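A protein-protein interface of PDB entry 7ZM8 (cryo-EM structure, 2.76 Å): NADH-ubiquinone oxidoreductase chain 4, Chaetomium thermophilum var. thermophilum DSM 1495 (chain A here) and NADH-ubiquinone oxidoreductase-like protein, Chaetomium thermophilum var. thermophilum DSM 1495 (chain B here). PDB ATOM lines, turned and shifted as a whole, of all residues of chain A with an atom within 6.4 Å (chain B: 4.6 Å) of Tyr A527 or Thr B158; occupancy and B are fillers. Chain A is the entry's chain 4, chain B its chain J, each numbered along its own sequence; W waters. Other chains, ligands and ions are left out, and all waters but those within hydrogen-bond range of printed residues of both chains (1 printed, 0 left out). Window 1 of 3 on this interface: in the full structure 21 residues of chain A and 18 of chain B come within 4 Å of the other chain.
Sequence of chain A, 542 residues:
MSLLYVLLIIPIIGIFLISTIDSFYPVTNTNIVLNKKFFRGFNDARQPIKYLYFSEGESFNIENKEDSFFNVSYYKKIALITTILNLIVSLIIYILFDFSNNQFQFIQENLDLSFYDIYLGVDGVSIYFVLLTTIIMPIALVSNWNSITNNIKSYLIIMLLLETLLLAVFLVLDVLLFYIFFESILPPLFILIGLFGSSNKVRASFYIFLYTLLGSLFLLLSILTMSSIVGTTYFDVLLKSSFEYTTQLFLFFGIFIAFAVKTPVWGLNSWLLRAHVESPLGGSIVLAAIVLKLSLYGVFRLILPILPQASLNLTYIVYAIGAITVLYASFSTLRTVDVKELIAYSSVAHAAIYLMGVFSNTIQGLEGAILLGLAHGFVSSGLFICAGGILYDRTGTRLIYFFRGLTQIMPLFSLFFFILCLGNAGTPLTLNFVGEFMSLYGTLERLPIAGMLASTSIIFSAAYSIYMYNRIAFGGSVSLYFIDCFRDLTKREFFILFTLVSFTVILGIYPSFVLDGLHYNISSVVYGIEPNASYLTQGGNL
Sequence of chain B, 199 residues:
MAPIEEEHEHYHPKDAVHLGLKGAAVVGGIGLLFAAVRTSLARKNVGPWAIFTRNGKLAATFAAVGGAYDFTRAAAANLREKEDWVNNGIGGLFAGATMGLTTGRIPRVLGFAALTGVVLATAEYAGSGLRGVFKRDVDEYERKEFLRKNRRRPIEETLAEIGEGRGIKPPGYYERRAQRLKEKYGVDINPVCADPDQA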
ATOM      1  N   LEU A 304     -18.395  15.874 -21.892  1.00  0.00           N
ATOM      2  CA  LEU A 304     -19.176  16.292 -20.700  1.00  0.00           C
ATOM      3  C   LEU A 304     -18.903  17.742 -20.292  1.00  0.00           C
ATOM      4  O   LEU A 304     -19.869  18.429 -19.962  1.00  0.00           O
ATOM      5  CB  LEU A 304     -18.958  15.281 -19.577  1.00  0.00           C
ATOM      6  CG  LEU A 304     -19.393  13.855 -19.894  1.00  0.00           C
ATOM      7  CD1 LEU A 304     -19.231  12.966 -18.678  1.00  0.00           C
ATOM      8  CD2 LEU A 304     -20.821  13.827 -20.411  1.00  0.00           C
ATOM      9  N   PRO A 308     -21.903  20.507 -23.357  1.00  0.00           N
ATOM     10  CA  PRO A 308     -23.046  20.058 -22.546  1.00  0.00           C
ATOM     11  C   PRO A 308     -24.439  20.128 -23.179  1.00  0.00           C
ATOM     12  O   PRO A 308     -25.182  19.209 -23.004  1.00  0.00           O
ATOM     13  CB  PRO A 308     -23.003  21.049 -21.386  1.00  0.00           C
ATOM     14  CG  PRO A 308     -22.484  22.302 -21.984  1.00  0.00           C
ATOM     15  CD  PRO A 308     -21.334  21.753 -22.781  1.00  0.00           C
ATOM     16  N   GLN A 309     -24.761  21.221 -23.858  1.00  0.00           N
ATOM     17  CA  GLN A 309     -26.071  21.427 -24.514  1.00  0.00           C
ATOM     18  C   GLN A 309     -26.267  20.406 -25.628  1.00  0.00           C
ATOM     19  O   GLN A 309     -27.388  19.921 -25.790  1.00  0.00           O
ATOM     20  CB  GLN A 309     -26.097  22.870 -24.984  1.00  0.00           C
ATOM     21  CG  GLN A 309     -25.994  23.860 -23.837  1.00  0.00           C
ATOM     22  CD  GLN A 309     -25.761  25.276 -24.299  1.00  0.00           C
ATOM     23  OE1 GLN A 309     -26.150  25.667 -25.394  1.00  0.00           O
ATOM     24  NE2 GLN A 309     -25.126  26.060 -23.448  1.00  0.00           N
ATOM     25  N   LEU A 312     -26.919  17.003 -24.000  1.00  0.00           N
ATOM     26  CA  LEU A 312     -28.312  16.972 -23.477  1.00  0.00           C
ATOM     27  C   LEU A 312     -29.344  16.763 -24.589  1.00  0.00           C
ATOM     28  O   LEU A 312     -30.166  15.847 -24.445  1.00  0.00           O
ATOM     29  CB  LEU A 312     -28.598  18.286 -22.747  1.00  0.00           C
ATOM     30  CG  LEU A 312     -29.750  18.254 -21.746  1.00  0.00           C
ATOM     31  CD1 LEU A 312     -29.525  17.178 -20.697  1.00  0.00           C
ATOM     32  CD2 LEU A 312     -29.918  19.607 -21.081  1.00  0.00           C
ATOM     33  N   ASN A 361     -26.076  12.530 -17.104  1.00  0.00           N
ATOM     34  CA  ASN A 361     -26.069  13.850 -16.423  1.00  0.00           C
ATOM     35  C   ASN A 361     -26.348  13.609 -14.953  1.00  0.00           C
ATOM     36  O   ASN A 361     -26.896  14.494 -14.295  1.00  0.00           O
ATOM     37  CB  ASN A 361     -26.969  14.892 -17.089  1.00  0.00           C
ATOM     38  CG  ASN A 361     -26.297  16.236 -17.226  1.00  0.00           C
ATOM     39  OD1 ASN A 361     -25.143  16.393 -16.849  1.00  0.00           O
ATOM     40  ND2 ASN A 361     -27.014  17.203 -17.767  1.00  0.00           N
ATOM     41  N   VAL A 525     -18.305  17.411 -13.793  1.00  0.00           N
ATOM     42  CA  VAL A 525     -18.765  17.154 -15.197  1.00  0.00           C
ATOM     43  C   VAL A 525     -20.294  17.136 -15.307  1.00  0.00           C
ATOM     44  O   VAL A 525     -20.775  16.823 -16.393  1.00  0.00           O
ATOM     45  CB  VAL A 525     -18.138  15.894 -15.835  1.00  0.00           C
ATOM     46  CG1 VAL A 525     -16.702  16.116 -16.275  1.00  0.00           C
ATOM     47  CG2 VAL A 525     -18.261  14.663 -14.955  1.00  0.00           C
ATOM     48  N   VAL A 526     -21.021  17.456 -14.236  1.00  0.00           N
ATOM     49  CA  VAL A 526     -22.518  17.450 -14.254  1.00  0.00           C
ATOM     50  C   VAL A 526     -23.005  18.774 -14.831  1.00  0.00           C
ATOM     51  O   VAL A 526     -22.411  19.793 -14.484  1.00  0.00           O
ATOM     52  CB  VAL A 526     -23.173  17.041 -12.922  1.00  0.00           C
ATOM     53  CG1 VAL A 526     -24.682  16.922 -13.052  1.00  0.00           C
ATOM     54  CG2 VAL A 526     -22.586  15.752 -12.379  1.00  0.00           C
ATOM     55  N   TYR A 527     -24.036  18.745 -15.673  1.00  0.00           N
ATOM     56  CA  TYR A 527     -24.620  19.994 -16.214  1.00  0.00           C
ATOM     57  C   TYR A 527     -26.041  20.142 -15.684  1.00  0.00           C
ATOM     58  O   TYR A 527     -26.884  19.290 -15.944  1.00  0.00           O
ATOM     59  CB  TYR A 527     -24.524  20.025 -17.735  1.00  0.00           C
ATOM     60  CG  TYR A 527     -24.863  21.314 -18.435  1.00  0.00           C
ATOM     61  CD1 TYR A 527     -24.023  22.408 -18.358  1.00  0.00           C
ATOM     62  CD2 TYR A 527     -25.982  21.409 -19.243  1.00  0.00           C
ATOM     63  CE1 TYR A 527     -24.304  23.577 -19.041  1.00  0.00           C
ATOM     64  CE2 TYR A 527     -26.281  22.571 -19.932  1.00  0.00           C
ATOM     65  CZ  TYR A 527     -25.438  23.660 -19.828  1.00  0.00           C
ATOM     66  OH  TYR A 527     -25.719  24.819 -20.487  1.00  0.00           O
ATOM     67  N   GLY A 528     -26.291  21.217 -14.962  1.00  0.00           N
ATOM     68  CA  GLY A 528     -27.645  21.489 -14.497  1.00  0.00           C
ATOM     69  C   GLY A 528     -27.683  22.362 -13.283  1.00  0.00           C
ATOM     70  O   GLY A 528     -26.659  22.538 -12.657  1.00  0.00           O
ATOM     71  N   ILE A 529     -28.846  22.902 -12.984  1.00  0.00           N
ATOM     72  CA  ILE A 529     -29.070  23.692 -11.783  1.00  0.00           C
ATOM     73  C   ILE A 529     -30.333  23.198 -11.102  1.00  0.00           C
ATOM     74  O   ILE A 529     -31.172  22.529 -11.704  1.00  0.00           O
ATOM     75  CB  ILE A 529     -29.194  25.205 -12.066  1.00  0.00           C
ATOM     76  CG1 ILE A 529     -30.080  25.455 -13.281  1.00  0.00           C
ATOM     77  CG2 ILE A 529     -27.825  25.843 -12.236  1.00  0.00           C
ATOM     78  CD1 ILE A 529     -30.386  26.899 -13.492  1.00  0.00           C
ATOM     79  N   PRO B 154     -26.332  34.930 -21.409  1.00  0.00           N
ATOM     80  CA  PRO B 154     -27.617  35.138 -20.743  1.00  0.00           C
ATOM     81  C   PRO B 154     -28.309  33.793 -20.475  1.00  0.00           C
ATOM     82  O   PRO B 154     -28.235  32.924 -21.299  1.00  0.00           O
ATOM     83  CB  PRO B 154     -28.406  35.860 -21.829  1.00  0.00           C
ATOM     84  CG  PRO B 154     -27.370  36.661 -22.559  1.00  0.00           C
ATOM     85  CD  PRO B 154     -26.185  35.728 -22.629  1.00  0.00           C
ATOM     86  N   ILE B 155     -28.991  33.666 -19.338  1.00  0.00           N
ATOM     87  CA  ILE B 155     -29.719  32.438 -19.048  1.00  0.00           C
ATOM     88  C   ILE B 155     -30.785  32.182 -20.101  1.00  0.00           C
ATOM     89  O   ILE B 155     -31.078  31.027 -20.429  1.00  0.00           O
ATOM     90  CB  ILE B 155     -30.314  32.507 -17.629  1.00  0.00           C
ATOM     91  CG1 ILE B 155     -30.843  31.146 -17.212  1.00  0.00           C
ATOM     92  CG2 ILE B 155     -31.404  33.564 -17.537  1.00  0.00           C
ATOM     93  CD1 ILE B 155     -29.784  30.137 -17.103  1.00  0.00           C
ATOM     94  N   GLU B 156     -31.383  33.240 -20.632  1.00  0.00           N
ATOM     95  CA  GLU B 156     -32.487  33.107 -21.614  1.00  0.00           C
ATOM     96  C   GLU B 156     -31.943  32.483 -22.888  1.00  0.00           C
ATOM     97  O   GLU B 156     -32.637  31.692 -23.499  1.00  0.00           O
ATOM     98  CB  GLU B 156     -33.023  34.499 -21.932  1.00  0.00           C
ATOM     99  CG  GLU B 156     -33.645  35.204 -20.740  1.00  0.00           C
ATOM    100  CD  GLU B 156     -32.674  35.955 -19.846  1.00  0.00           C
ATOM    101  OE1 GLU B 156     -31.481  36.033 -20.201  1.00  0.00           O
ATOM    102  OE2 GLU B 156     -33.113  36.456 -18.792  1.00  0.00           O
ATOM    103  N   GLU B 157     -30.727  32.846 -23.260  1.00  0.00           N
ATOM    104  CA  GLU B 157     -30.082  32.320 -24.479  1.00  0.00           C
ATOM    105  C   GLU B 157     -30.001  30.788 -24.438  1.00  0.00           C
ATOM    106  O   GLU B 157     -30.297  30.169 -25.470  1.00  0.00           O
ATOM    107  CB  GLU B 157     -28.707  32.976 -24.616  1.00  0.00           C
ATOM    108  CG  GLU B 157     -27.976  32.561 -25.879  1.00  0.00           C
ATOM    109  CD  GLU B 157     -26.739  33.369 -26.220  1.00  0.00           C
ATOM    110  OE1 GLU B 157     -25.982  32.938 -27.113  1.00  0.00           O
ATOM    111  OE2 GLU B 157     -26.539  34.432 -25.603  1.00  0.00           O
ATOM    112  N   THR B 158     -29.583  30.201 -23.319  1.00  0.00           N
ATOM    113  CA  THR B 158     -29.395  28.731 -23.252  1.00  0.00           C
ATOM    114  C   THR B 158     -30.747  28.034 -23.143  1.00  0.00           C
ATOM    115  O   THR B 158     -30.913  27.003 -23.800  1.00  0.00           O
ATOM    116  CB  THR B 158     -28.459  28.335 -22.106  1.00  0.00           C
ATOM    117  OG1 THR B 158     -27.216  28.999 -22.333  1.00  0.00           O
ATOM    118  CG2 THR B 158     -28.225  26.845 -21.994  1.00  0.00           C
ATOM    119  N   LEU B 159     -31.707  28.625 -22.430  1.00  0.00           N
ATOM    120  CA  LEU B 159     -33.011  27.966 -22.174  1.00  0.00           C
ATOM    121  C   LEU B 159     -33.781  27.913 -23.477  1.00  0.00           C
ATOM    122  O   LEU B 159     -34.820  27.248 -23.530  1.00  0.00           O
ATOM    123  CB  LEU B 159     -33.780  28.753 -21.114  1.00  0.00           C
ATOM    124  CG  LEU B 159     -33.210  28.660 -19.700  1.00  0.00           C
ATOM    125  CD1 LEU B 159     -34.049  29.455 -18.717  1.00  0.00           C
ATOM    126  CD2 LEU B 159     -33.090  27.211 -19.259  1.00  0.00           C
ATOM    127  N   ALA B 160     -33.276  28.599 -24.489  1.00  0.00           N
ATOM    128  CA  ALA B 160     -33.968  28.673 -25.784  1.00  0.00           C
ATOM    129  C   ALA B 160     -33.601  27.415 -26.568  1.00  0.00           C
ATOM    130  O   ALA B 160     -34.481  26.838 -27.228  1.00  0.00           O
ATOM    131  CB  ALA B 160     -33.530  29.926 -26.488  1.00  0.00           C
ATOM    132  N   GLU B 161     -32.332  27.012 -26.474  1.00  0.00           N
ATOM    133  CA  GLU B 161     -31.884  25.812 -27.236  1.00  0.00           C
ATOM    134  C   GLU B 161     -32.210  24.509 -26.506  1.00  0.00           C
ATOM    135  O   GLU B 161     -32.619  23.564 -27.187  1.00  0.00           O
ATOM    136  CB  GLU B 161     -30.403  25.901 -27.619  1.00  0.00           C
ATOM    137  CG  GLU B 161     -30.045  27.151 -28.397  1.00  0.00           C
ATOM    138  CD  GLU B 161     -30.395  27.108 -29.874  1.00  0.00           C
ATOM    139  OE1 GLU B 161     -30.896  26.063 -30.333  1.00  0.00           O
ATOM    140  OE2 GLU B 161     -30.159  28.119 -30.563  1.00  0.00           O
ATOM    141  N   ILE B 162     -31.978  24.449 -25.193  1.00  0.00           N
ATOM    142  CA  ILE B 162     -32.204  23.169 -24.476  1.00  0.00           C
ATOM    143  C   ILE B 162     -33.602  23.187 -23.862  1.00  0.00           C
ATOM    144  O   ILE B 162     -34.314  22.191 -24.025  1.00  0.00           O
ATOM    145  CB  ILE B 162     -31.091  22.858 -23.453  1.00  0.00           C
ATOM    146  CG1 ILE B 162     -30.815  24.021 -22.498  1.00  0.00           C
ATOM    147  CG2 ILE B 162     -29.832  22.396 -24.165  1.00  0.00           C
ATOM    148  CD1 ILE B 162     -29.994  23.636 -21.297  1.00  0.00           C
ATOM    149  N   GLY B 163     -33.956  24.245 -23.146  1.00  0.00           N
ATOM    150  CA  GLY B 163     -35.259  24.311 -22.462  1.00  0.00           C
ATOM    151  C   GLY B 163     -35.148  23.906 -21.009  1.00  0.00           C
ATOM    152  O   GLY B 163     -34.204  23.178 -20.671  1.00  0.00           O
ATOM    153  N   ILE B 168     -32.510  20.785 -15.736  1.00  0.00           N
ATOM    154  CA  ILE B 168     -32.260  22.240 -15.892  1.00  0.00           C
ATOM    155  C   ILE B 168     -33.437  22.916 -15.215  1.00  0.00           C
ATOM    156  O   ILE B 168     -34.433  23.182 -15.892  1.00  0.00           O
ATOM    157  CB  ILE B 168     -32.139  22.636 -17.375  1.00  0.00           C
ATOM    158  CG1 ILE B 168     -31.150  21.734 -18.117  1.00  0.00           C
ATOM    159  CG2 ILE B 168     -31.764  24.103 -17.510  1.00  0.00           C
ATOM    160  CD1 ILE B 168     -29.713  21.925 -17.698  1.00  0.00           C
HETATM  161  O   HOH W   1     -24.133  28.557 -22.555  1.00  0.00           O
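The side-chain amide nitrogen of Gln A309 lies within hydrogen-bond range of the side-chain hydroxyl of Tyr A527. O of Tyr A527 sits at hydrogen-bond distance from ND2 of Asn A361.
Thr B158 touches Gln A309. O of Gln A309 touches CG2 of Ile B162, 3.8 Å away. Ile B168 touches Leu A312. Thr B158 touches Tyr A527. CA of Gly A528 touches CD1 of Ile B168, 3.8 Å away.
Of the printed residues of chain B, Gln A309 touches Thr B158 (3.5 Å) and Ile B162 (3.8 Å). Of the printed residues of chain B, Leu A312 touches Ile B168 (3.9 Å). Printed residues of chain B within 4 Å of Gly A528: Ile B168. Glu B157 touches none of the printed residues of chain A. Thr B158 touches just these residues of chain A: Gln A309 (3.5 Å) and Tyr A527 (3.6 Å). Printed residues of chain A within 4 Å of Ile B162: Gln A309 (3.8 Å). Of the printed residues of chain A, Ile B168 touches Leu A312 and Gly A528. The nearest printed residue of chain B that does not touch Gly A528 is Ile B162 (7.5 Å).
Of the 11 printed residues of chain B, 3 touch a printed residue of chain A. Printed residues of chain B that touch a printed residue of chain A: Thr B158, Ile B162 and Ile B168. Of the 10 printed residues of chain A, 4 touch a printed residue of chain B. Among the printed residues, no Asp or Glu carboxylate lies within 4 Å of a Lys or Arg side-chain nitrogen of the other chain.
Water W1 lies within hydrogen-bond range of the side-chain amide nitrogen (NE2) of Gln A309 and the side-chain hydroxyl (OG1) of Thr B158.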
